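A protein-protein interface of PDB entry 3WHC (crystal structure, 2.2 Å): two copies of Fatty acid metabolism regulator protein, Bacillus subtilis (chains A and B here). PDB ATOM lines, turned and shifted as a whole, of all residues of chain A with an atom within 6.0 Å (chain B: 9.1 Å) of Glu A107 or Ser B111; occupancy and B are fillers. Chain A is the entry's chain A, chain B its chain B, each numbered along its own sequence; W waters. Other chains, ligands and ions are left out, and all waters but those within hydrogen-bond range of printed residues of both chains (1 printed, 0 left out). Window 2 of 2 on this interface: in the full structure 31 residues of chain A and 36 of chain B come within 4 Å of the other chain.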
ATOM      1  N   ILE A  19     -33.249   4.391  27.050  1.00  0.00           N
ATOM      2  CA  ILE A  19     -31.926   4.202  26.444  1.00  0.00           C
ATOM      3  C   ILE A  19     -30.973   3.449  27.381  1.00  0.00           C
ATOM      4  O   ILE A  19     -30.185   2.611  26.933  1.00  0.00           O
ATOM      5  CB  ILE A  19     -31.319   5.544  25.963  1.00  0.00           C
ATOM      6  CG1 ILE A  19     -32.184   6.145  24.850  1.00  0.00           C
ATOM      7  CG2 ILE A  19     -29.894   5.354  25.457  1.00  0.00           C
ATOM      8  CD1 ILE A  19     -31.965   7.626  24.612  1.00  0.00           C
ATOM      9  N   ALA A  20     -31.064   3.731  28.678  1.00  0.00           N
ATOM     10  CA  ALA A  20     -30.252   3.034  29.676  1.00  0.00           C
ATOM     11  C   ALA A  20     -30.653   1.565  29.829  1.00  0.00           C
ATOM     12  O   ALA A  20     -29.788   0.691  29.912  1.00  0.00           O
ATOM     13  CB  ALA A  20     -30.321   3.749  31.017  1.00  0.00           C
ATOM     14  N   ASN A  22     -32.566  -0.294  27.649  1.00  0.00           N
ATOM     15  CA  ASN A  22     -32.690  -1.021  26.383  1.00  0.00           C
ATOM     16  C   ASN A  22     -31.444  -0.968  25.504  1.00  0.00           C
ATOM     17  O   ASN A  22     -31.149  -1.919  24.781  1.00  0.00           O
ATOM     18  CB  ASN A  22     -33.885  -0.497  25.574  1.00  0.00           C
ATOM     19  CG  ASN A  22     -35.227  -0.884  26.172  1.00  0.00           C
ATOM     20  OD1 ASN A  22     -36.054  -1.500  25.502  1.00  0.00           O
ATOM     21  ND2 ASN A  22     -35.457  -0.510  27.427  1.00  0.00           N
ATOM     22  N   GLY A  23     -30.723   0.149  25.567  1.00  0.00           N
ATOM     23  CA  GLY A  23     -29.653   0.437  24.616  1.00  0.00           C
ATOM     24  C   GLY A  23     -30.194   1.309  23.498  1.00  0.00           C
ATOM     25  O   GLY A  23     -31.361   1.183  23.119  1.00  0.00           O
ATOM     26  N   TYR A  24     -29.345   2.188  22.969  1.00  0.00           N
ATOM     27  CA  TYR A  24     -29.754   3.167  21.956  1.00  0.00           C
ATOM     28  C   TYR A  24     -30.338   2.540  20.687  1.00  0.00           C
ATOM     29  O   TYR A  24     -31.313   3.058  20.135  1.00  0.00           O
ATOM     30  CB  TYR A  24     -28.591   4.105  21.606  1.00  0.00           C
ATOM     31  CG  TYR A  24     -28.914   5.105  20.515  1.00  0.00           C
ATOM     32  CD1 TYR A  24     -29.868   6.103  20.716  1.00  0.00           C
ATOM     33  CD2 TYR A  24     -28.266   5.053  19.282  1.00  0.00           C
ATOM     34  CE1 TYR A  24     -30.167   7.020  19.720  1.00  0.00           C
ATOM     35  CE2 TYR A  24     -28.557   5.966  18.280  1.00  0.00           C
ATOM     36  CZ  TYR A  24     -29.509   6.947  18.505  1.00  0.00           C
ATOM     37  OH  TYR A  24     -29.806   7.853  17.515  1.00  0.00           O
ATOM     38  N   HIS A  25     -29.746   1.436  20.234  1.00  0.00           N
ATOM     39  CA  HIS A  25     -30.227   0.719  19.048  1.00  0.00           C
ATOM     40  C   HIS A  25     -31.672   0.241  19.201  1.00  0.00           C
ATOM     41  O   HIS A  25     -32.454   0.297  18.251  1.00  0.00           O
ATOM     42  CB  HIS A  25     -29.323  -0.478  18.719  1.00  0.00           C
ATOM     43  CG  HIS A  25     -27.989  -0.101  18.148  1.00  0.00           C
ATOM     44  ND1 HIS A  25     -27.830   0.912  17.226  1.00  0.00           N
ATOM     45  CD2 HIS A  25     -26.756  -0.626  18.346  1.00  0.00           C
ATOM     46  CE1 HIS A  25     -26.554   1.006  16.895  1.00  0.00           C
ATOM     47  NE2 HIS A  25     -25.881   0.083  17.559  1.00  0.00           N
ATOM     48  N   LEU A  54     -31.906  11.830  21.537  1.00  0.00           N
ATOM     49  CA  LEU A  54     -30.607  11.564  22.171  1.00  0.00           C
ATOM     50  C   LEU A  54     -29.755  12.825  22.320  1.00  0.00           C
ATOM     51  O   LEU A  54     -29.192  13.077  23.391  1.00  0.00           O
ATOM     52  CB  LEU A  54     -29.828  10.486  21.406  1.00  0.00           C
ATOM     53  CG  LEU A  54     -28.485  10.048  22.004  1.00  0.00           C
ATOM     54  CD1 LEU A  54     -28.678   9.114  23.194  1.00  0.00           C
ATOM     55  CD2 LEU A  54     -27.601   9.396  20.951  1.00  0.00           C
ATOM     56  N   ILE A 102     -24.990   5.182  32.577  1.00  0.00           N
ATOM     57  CA  ILE A 102     -25.062   4.248  31.446  1.00  0.00           C
ATOM     58  C   ILE A 102     -25.128   5.013  30.119  1.00  0.00           C
ATOM     59  O   ILE A 102     -24.440   4.662  29.156  1.00  0.00           O
ATOM     60  CB  ILE A 102     -26.254   3.268  31.584  1.00  0.00           C
ATOM     61  CG1 ILE A 102     -25.979   2.257  32.705  1.00  0.00           C
ATOM     62  CG2 ILE A 102     -26.520   2.532  30.274  1.00  0.00           C
ATOM     63  CD1 ILE A 102     -27.212   1.550  33.233  1.00  0.00           C
ATOM     64  N   VAL A 103     -25.945   6.065  30.088  1.00  0.00           N
ATOM     65  CA  VAL A 103     -26.076   6.911  28.904  1.00  0.00           C
ATOM     66  C   VAL A 103     -24.754   7.621  28.582  1.00  0.00           C
ATOM     67  O   VAL A 103     -24.305   7.592  27.439  1.00  0.00           O
ATOM     68  CB  VAL A 103     -27.240   7.925  29.037  1.00  0.00           C
ATOM     69  CG1 VAL A 103     -27.337   8.807  27.800  1.00  0.00           C
ATOM     70  CG2 VAL A 103     -28.562   7.202  29.258  1.00  0.00           C
ATOM     71  N   THR A 104     -24.124   8.224  29.589  1.00  0.00           N
ATOM     72  CA  THR A 104     -22.888   8.992  29.371  1.00  0.00           C
ATOM     73  C   THR A 104     -21.657   8.143  29.023  1.00  0.00           C
ATOM     74  O   THR A 104     -20.879   8.523  28.144  1.00  0.00           O
ATOM     75  CB  THR A 104     -22.539   9.928  30.552  1.00  0.00           C
ATOM     76  OG1 THR A 104     -22.363   9.162  31.750  1.00  0.00           O
ATOM     77  CG2 THR A 104     -23.631  10.969  30.768  1.00  0.00           C
ATOM     78  N   GLN A 105     -21.489   7.009  29.706  1.00  0.00           N
ATOM     79  CA  GLN A 105     -20.286   6.169  29.542  1.00  0.00           C
ATOM     80  C   GLN A 105     -20.385   5.150  28.410  1.00  0.00           C
ATOM     81  O   GLN A 105     -19.360   4.714  27.877  1.00  0.00           O
ATOM     82  CB  GLN A 105     -19.930   5.434  30.843  1.00  0.00           C
ATOM     83  CG  GLN A 105     -19.798   6.314  32.078  1.00  0.00           C
ATOM     84  CD  GLN A 105     -19.028   7.597  31.822  1.00  0.00           C
ATOM     85  OE1 GLN A 105     -19.613   8.675  31.761  1.00  0.00           O
ATOM     86  NE2 GLN A 105     -17.716   7.486  31.670  1.00  0.00           N
ATOM     87  N   LEU A 106     -21.608   4.762  28.059  1.00  0.00           N
ATOM     88  CA  LEU A 106     -21.814   3.731  27.043  1.00  0.00           C
ATOM     89  C   LEU A 106     -22.654   4.200  25.859  1.00  0.00           C
ATOM     90  O   LEU A 106     -22.203   4.144  24.713  1.00  0.00           O
ATOM     91  CB  LEU A 106     -22.413   2.461  27.666  1.00  0.00           C
ATOM     92  CG  LEU A 106     -21.574   1.692  28.698  1.00  0.00           C
ATOM     93  CD1 LEU A 106     -22.424   0.658  29.426  1.00  0.00           C
ATOM     94  CD2 LEU A 106     -20.359   1.034  28.056  1.00  0.00           C
ATOM     95  N   GLU A 107     -23.865   4.674  26.137  1.00  0.00           N
ATOM     96  CA  GLU A 107     -24.852   4.923  25.086  1.00  0.00           C
ATOM     97  C   GLU A 107     -24.589   6.144  24.203  1.00  0.00           C
ATOM     98  O   GLU A 107     -24.979   6.160  23.034  1.00  0.00           O
ATOM     99  CB  GLU A 107     -26.267   4.953  25.669  1.00  0.00           C
ATOM    100  CG  GLU A 107     -26.705   3.636  26.306  1.00  0.00           C
ATOM    101  CD  GLU A 107     -26.614   2.451  25.357  1.00  0.00           C
ATOM    102  OE1 GLU A 107     -27.022   2.581  24.186  1.00  0.00           O
ATOM    103  OE2 GLU A 107     -26.133   1.381  25.783  1.00  0.00           O
ATOM    104  N   LEU A 108     -23.927   7.156  24.760  1.00  0.00           N
ATOM    105  CA  LEU A 108     -23.580   8.364  24.006  1.00  0.00           C
ATOM    106  C   LEU A 108     -22.286   8.224  23.204  1.00  0.00           C
ATOM    107  O   LEU A 108     -21.912   9.135  22.460  1.00  0.00           O
ATOM    108  CB  LEU A 108     -23.502   9.583  24.934  1.00  0.00           C
ATOM    109  CG  LEU A 108     -24.834  10.235  25.317  1.00  0.00           C
ATOM    110  CD1 LEU A 108     -24.647  11.183  26.493  1.00  0.00           C
ATOM    111  CD2 LEU A 108     -25.452  10.961  24.129  1.00  0.00           C
ATOM    112  N   ARG A 109     -21.617   7.081  23.350  1.00  0.00           N
ATOM    113  CA  ARG A 109     -20.342   6.828  22.685  1.00  0.00           C
ATOM    114  C   ARG A 109     -20.595   6.278  21.285  1.00  0.00           C
ATOM    115  O   ARG A 109     -20.310   5.113  20.995  1.00  0.00           O
ATOM    116  CB  ARG A 109     -19.489   5.855  23.509  1.00  0.00           C
ATOM    117  CG  ARG A 109     -19.471   6.144  25.003  1.00  0.00           C
ATOM    118  CD  ARG A 109     -18.336   7.074  25.391  1.00  0.00           C
ATOM    119  NE  ARG A 109     -18.609   7.788  26.635  1.00  0.00           N
ATOM    120  CZ  ARG A 109     -17.671   8.238  27.467  1.00  0.00           C
ATOM    121  NH1 ARG A 109     -16.382   8.038  27.205  1.00  0.00           N
ATOM    122  NH2 ARG A 109     -18.023   8.882  28.567  1.00  0.00           N
ATOM    123  N   GLN A 110     -21.135   7.133  20.422  1.00  0.00           N
ATOM    124  CA  GLN A 110     -21.558   6.727  19.086  1.00  0.00           C
ATOM    125  C   GLN A 110     -20.418   6.741  18.076  1.00  0.00           C
ATOM    126  O   GLN A 110     -19.629   7.688  18.027  1.00  0.00           O
ATOM    127  CB  GLN A 110     -22.725   7.594  18.601  1.00  0.00           C
ATOM    128  CG  GLN A 110     -24.032   7.341  19.345  1.00  0.00           C
ATOM    129  CD  GLN A 110     -24.508   5.900  19.241  1.00  0.00           C
ATOM    130  OE1 GLN A 110     -24.438   5.283  18.178  1.00  0.00           O
ATOM    131  NE2 GLN A 110     -24.994   5.357  20.352  1.00  0.00           N
ATOM    132  N   TYR B  24     -18.290  -0.607  12.486  1.00  0.00           N
ATOM    133  CA  TYR B  24     -18.353  -2.038  12.783  1.00  0.00           C
ATOM    134  C   TYR B  24     -19.689  -2.674  12.392  1.00  0.00           C
ATOM    135  O   TYR B  24     -19.712  -3.670  11.669  1.00  0.00           O
ATOM    136  CB  TYR B  24     -18.040  -2.313  14.261  1.00  0.00           C
ATOM    137  CG  TYR B  24     -18.384  -3.722  14.696  1.00  0.00           C
ATOM    138  CD1 TYR B  24     -17.675  -4.817  14.200  1.00  0.00           C
ATOM    139  CD2 TYR B  24     -19.425  -3.962  15.592  1.00  0.00           C
ATOM    140  CE1 TYR B  24     -17.990  -6.107  14.582  1.00  0.00           C
ATOM    141  CE2 TYR B  24     -19.747  -5.252  15.983  1.00  0.00           C
ATOM    142  CZ  TYR B  24     -19.024  -6.318  15.473  1.00  0.00           C
ATOM    143  OH  TYR B  24     -19.328  -7.600  15.850  1.00  0.00           O
ATOM    144  N   HIS B  25     -20.790  -2.098  12.866  1.00  0.00           N
ATOM    145  CA  HIS B  25     -22.116  -2.676  12.643  1.00  0.00           C
ATOM    146  C   HIS B  25     -22.571  -2.617  11.188  1.00  0.00           C
ATOM    147  O   HIS B  25     -23.264  -3.517  10.708  1.00  0.00           O
ATOM    148  CB  HIS B  25     -23.148  -2.029  13.564  1.00  0.00           C
ATOM    149  CG  HIS B  25     -23.020  -2.457  14.992  1.00  0.00           C
ATOM    150  ND1 HIS B  25     -23.260  -3.751  15.403  1.00  0.00           N
ATOM    151  CD2 HIS B  25     -22.672  -1.766  16.103  1.00  0.00           C
ATOM    152  CE1 HIS B  25     -23.069  -3.838  16.707  1.00  0.00           C
ATOM    153  NE2 HIS B  25     -22.713  -2.649  17.156  1.00  0.00           N
ATOM    154  N   LEU B 106     -13.124   4.662  18.339  1.00  0.00           N
ATOM    155  CA  LEU B 106     -14.535   4.759  17.964  1.00  0.00           C
ATOM    156  C   LEU B 106     -15.231   3.410  17.815  1.00  0.00           C
ATOM    157  O   LEU B 106     -16.301   3.195  18.389  1.00  0.00           O
ATOM    158  CB  LEU B 106     -14.707   5.597  16.687  1.00  0.00           C
ATOM    159  CG  LEU B 106     -14.279   7.074  16.720  1.00  0.00           C
ATOM    160  CD1 LEU B 106     -14.276   7.679  15.322  1.00  0.00           C
ATOM    161  CD2 LEU B 106     -15.156   7.896  17.656  1.00  0.00           C
ATOM    162  N   GLU B 107     -14.621   2.502  17.058  1.00  0.00           N
ATOM    163  CA  GLU B 107     -15.282   1.248  16.683  1.00  0.00           C
ATOM    164  C   GLU B 107     -15.240   0.144  17.742  1.00  0.00           C
ATOM    165  O   GLU B 107     -16.136  -0.697  17.797  1.00  0.00           O
ATOM    166  CB  GLU B 107     -14.751   0.737  15.341  1.00  0.00           C
ATOM    167  CG  GLU B 107     -15.013   1.681  14.170  1.00  0.00           C
ATOM    168  CD  GLU B 107     -16.475   2.072  14.024  1.00  0.00           C
ATOM    169  OE1 GLU B 107     -17.361   1.226  14.270  1.00  0.00           O
ATOM    170  OE2 GLU B 107     -16.743   3.231  13.652  1.00  0.00           O
ATOM    171  N   LEU B 108     -14.206   0.143  18.577  1.00  0.00           N
ATOM    172  CA  LEU B 108     -14.113  -0.827  19.666  1.00  0.00           C
ATOM    173  C   LEU B 108     -14.868  -0.379  20.923  1.00  0.00           C
ATOM    174  O   LEU B 108     -14.857  -1.074  21.939  1.00  0.00           O
ATOM    175  CB  LEU B 108     -12.648  -1.137  19.990  1.00  0.00           C
ATOM    176  CG  LEU B 108     -11.924  -2.105  19.047  1.00  0.00           C
ATOM    177  CD1 LEU B 108     -10.425  -2.051  19.283  1.00  0.00           C
ATOM    178  CD2 LEU B 108     -12.436  -3.531  19.202  1.00  0.00           C
ATOM    179  N   ARG B 109     -15.529   0.773  20.844  1.00  0.00           N
ATOM    180  CA  ARG B 109     -16.247   1.350  21.983  1.00  0.00           C
ATOM    181  C   ARG B 109     -17.714   0.913  21.965  1.00  0.00           C
ATOM    182  O   ARG B 109     -18.626   1.744  21.960  1.00  0.00           O
ATOM    183  CB  ARG B 109     -16.137   2.879  21.965  1.00  0.00           C
ATOM    184  CG  ARG B 109     -14.742   3.408  21.654  1.00  0.00           C
ATOM    185  CD  ARG B 109     -13.945   3.717  22.911  1.00  0.00           C
ATOM    186  NE  ARG B 109     -12.508   3.731  22.646  1.00  0.00           N
ATOM    187  CZ  ARG B 109     -11.614   4.441  23.331  1.00  0.00           C
ATOM    188  NH1 ARG B 109     -11.996   5.226  24.334  1.00  0.00           N
ATOM    189  NH2 ARG B 109     -10.331   4.375  23.002  1.00  0.00           N
ATOM    190  N   GLN B 110     -17.924  -0.399  21.957  1.00  0.00           N
ATOM    191  CA  GLN B 110     -19.255  -0.985  21.827  1.00  0.00           C
ATOM    192  C   GLN B 110     -20.017  -0.981  23.149  1.00  0.00           C
ATOM    193  O   GLN B 110     -19.433  -1.224  24.207  1.00  0.00           O
ATOM    194  CB  GLN B 110     -19.146  -2.410  21.274  1.00  0.00           C
ATOM    195  CG  GLN B 110     -18.540  -2.483  19.879  1.00  0.00           C
ATOM    196  CD  GLN B 110     -19.368  -1.744  18.842  1.00  0.00           C
ATOM    197  OE1 GLN B 110     -20.588  -1.894  18.784  1.00  0.00           O
ATOM    198  NE2 GLN B 110     -18.706  -0.938  18.019  1.00  0.00           N
ATOM    199  N   SER B 111     -21.320  -0.712  23.078  1.00  0.00           N
ATOM    200  CA  SER B 111     -22.162  -0.591  24.277  1.00  0.00           C
ATOM    201  C   SER B 111     -22.736  -1.916  24.785  1.00  0.00           C
ATOM    202  O   SER B 111     -23.126  -2.011  25.952  1.00  0.00           O
ATOM    203  CB  SER B 111     -23.292   0.420  24.051  1.00  0.00           C
ATOM    204  OG  SER B 111     -24.102   0.050  22.952  1.00  0.00           O
ATOM    205  N   ASN B 112     -22.793  -2.925  23.916  1.00  0.00           N
ATOM    206  CA  ASN B 112     -23.266  -4.256  24.301  1.00  0.00           C
ATOM    207  C   ASN B 112     -22.361  -4.878  25.362  1.00  0.00           C
ATOM    208  O   ASN B 112     -21.174  -5.107  25.116  1.00  0.00           O
ATOM    209  CB  ASN B 112     -23.374  -5.180  23.077  1.00  0.00           C
ATOM    210  CG  ASN B 112     -23.920  -6.557  23.423  1.00  0.00           C
ATOM    211  OD1 ASN B 112     -23.241  -7.570  23.239  1.00  0.00           O
ATOM    212  ND2 ASN B 112     -25.148  -6.603  23.930  1.00  0.00           N
ATOM    213  N   LEU B 113     -22.936  -5.137  26.537  1.00  0.00           N
ATOM    214  CA  LEU B 113     -22.198  -5.661  27.694  1.00  0.00           C
ATOM    215  C   LEU B 113     -21.364  -6.898  27.368  1.00  0.00           C
ATOM    216  O   LEU B 113     -20.170  -6.948  27.675  1.00  0.00           O
ATOM    217  CB  LEU B 113     -23.156  -5.962  28.861  1.00  0.00           C
ATOM    218  CG  LEU B 113     -23.493  -4.889  29.915  1.00  0.00           C
ATOM    219  CD1 LEU B 113     -22.249  -4.413  30.661  1.00  0.00           C
ATOM    220  CD2 LEU B 113     -24.258  -3.708  29.328  1.00  0.00           C
ATOM    221  N   GLU B 114     -22.007  -7.881  26.741  1.00  0.00           N
ATOM    222  CA  GLU B 114     -21.372  -9.134  26.331  1.00  0.00           C
ATOM    223  C   GLU B 114     -20.121  -8.907  25.477  1.00  0.00           C
ATOM    224  O   GLU B 114     -19.052  -9.444  25.774  1.00  0.00           O
ATOM    225  CB  GLU B 114     -22.378  -9.995  25.560  1.00  0.00           C
ATOM    226  CG  GLU B 114     -23.452 -10.650  26.420  1.00  0.00           C
ATOM    227  CD  GLU B 114     -23.155 -12.108  26.732  1.00  0.00           C
ATOM    228  OE1 GLU B 114     -22.476 -12.771  25.917  1.00  0.00           O
ATOM    229  OE2 GLU B 114     -23.614 -12.595  27.788  1.00  0.00           O
ATOM    230  N   LEU B 115     -20.266  -8.102  24.426  1.00  0.00           N
ATOM    231  CA  LEU B 115     -19.175  -7.807  23.496  1.00  0.00           C
ATOM    232  C   LEU B 115     -18.089  -6.929  24.125  1.00  0.00           C
ATOM    233  O   LEU B 115     -16.895  -7.138  23.882  1.00  0.00           O
ATOM    234  CB  LEU B 115     -19.731  -7.156  22.221  1.00  0.00           C
ATOM    235  CG  LEU B 115     -18.809  -6.581  21.134  1.00  0.00           C
ATOM    236  CD1 LEU B 115     -17.774  -7.587  20.651  1.00  0.00           C
ATOM    237  CD2 LEU B 115     -19.639  -6.076  19.964  1.00  0.00           C
ATOM    238  N   ARG B 116     -18.510  -5.956  24.929  1.00  0.00           N
ATOM    239  CA  ARG B 116     -17.595  -4.996  25.547  1.00  0.00           C
ATOM    240  C   ARG B 116     -16.667  -5.642  26.583  1.00  0.00           C
ATOM    241  O   ARG B 116     -15.506  -5.241  26.720  1.00  0.00           O
ATOM    242  CB  ARG B 116     -18.386  -3.832  26.159  1.00  0.00           C
ATOM    243  CG  ARG B 116     -17.553  -2.744  26.825  1.00  0.00           C
ATOM    244  CD  ARG B 116     -16.583  -2.057  25.873  1.00  0.00           C
ATOM    245  NE  ARG B 116     -16.011  -0.864  26.494  1.00  0.00           N
ATOM    246  CZ  ARG B 116     -16.541   0.356  26.416  1.00  0.00           C
ATOM    247  NH1 ARG B 116     -15.951   1.373  27.027  1.00  0.00           N
ATOM    248  NH2 ARG B 116     -17.658   0.564  25.728  1.00  0.00           N
ATOM    249  N   GLN B 117     -17.185  -6.641  27.296  1.00  0.00           N
ATOM    250  CA  GLN B 117     -16.402  -7.399  28.275  1.00  0.00           C
ATOM    251  C   GLN B 117     -15.267  -8.190  27.617  1.00  0.00           C
ATOM    252  O   GLN B 117     -14.184  -8.314  28.187  1.00  0.00           O
ATOM    253  CB  GLN B 117     -17.304  -8.333  29.089  1.00  0.00           C
ATOM    254  CG  GLN B 117     -18.082  -7.641  30.200  1.00  0.00           C
ATOM    255  N   ILE B 119     -13.858  -7.243  24.787  1.00  0.00           N
ATOM    256  CA  ILE B 119     -12.956  -6.171  24.377  1.00  0.00           C
ATOM    257  C   ILE B 119     -12.076  -5.719  25.552  1.00  0.00           C
ATOM    258  O   ILE B 119     -10.850  -5.640  25.428  1.00  0.00           O
ATOM    259  CB  ILE B 119     -13.743  -4.978  23.771  1.00  0.00           C
ATOM    260  CG1 ILE B 119     -14.378  -5.384  22.435  1.00  0.00           C
ATOM    261  CG2 ILE B 119     -12.846  -3.755  23.602  1.00  0.00           C
ATOM    262  CD1 ILE B 119     -15.460  -4.446  21.934  1.00  0.00           C
HETATM  263  O   HOH W   1     -14.747   6.800  24.952  1.00  0.00           O
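Of the 15 printed residues of chain B, 4 touch a printed residue of chain A.
Hydrophobic or aromatic side chains of chain B within 4 Å of the printed part of chain A: His B25.
Of the 16 printed residues of chain A, 4 touch a printed residue of chain B.
Along chain A the printed residues that touch a printed residue of chain B span positions 25 to 109.
Among the printed residues, pairs that only touch across the chains: Glu A107 with Ser B111, Leu A106 with Arg B116, Arg A109 with Arg B109, Leu A106 with Ser B111 and His A25 with His B25.
Water W1 lies within hydrogen-bond range of the guanidinium group of Arg A109 (3.0 Å) and the guanidinium group of Arg B109 (3.2 Å).
His B25 touches its own counterpart, His A25.
Arg B109 touches its own counterpart, Arg A109.
Positions printed for both chains: 24, 25, 106, 107, 108, 109 and 110.
Of the 5 pairs that touch across the chains among the printed residues, 2 have their exchanged pair printed and touching as well.
Ser B111 touches two residues of chain A.
No residue of chain B comes within 4 Å of Gly A23.
No residue of chain B comes within 4 Å of Val A103.
Leu A106 touches just these residues of chain B: Ser B111 and Arg B116.
Of the printed residues of chain A, His B25 touches His A25.
Of the printed residues of chain B, His A25 touches His B25.
Of the printed residues of chain B, Arg A109 touches Arg B109 (3.9 Å).
Printed residues of chain A within 4 Å of Arg B116: Leu A106.
Leu A108 touches none of the printed residues of chain B.
Leu B113 touches none of the printed residues of chain A.
The nearest printed residue of chain B that does not touch Arg A109 is Leu B106 (5.2 Å).
The backbone NH of Tyr A24 lies within hydrogen-bond range of the side-chain carboxylate of Glu A107 (2.7 Å).
The backbone carbonyl oxygen (O) of Ile A102 lies within hydrogen-bond range of the backbone NH (N) of Glu A107 (3.1 Å).
The backbone carbonyl oxygen of Gln A105 lies close to the guanidinium group of Arg A109 (3.4 Å).
O of Glu A107 lies within hydrogen-bond range of NE2 of Gln A110, at 2.8 Å.
The side-chain amide oxygen of Gln B110 is in hydrogen-bond range of a ring nitrogen (NE2) of His B25 (2.8 Å).
NH2 of Arg B116 lies within hydrogen-bond range of O of Gln B110, 2.9 Å away.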
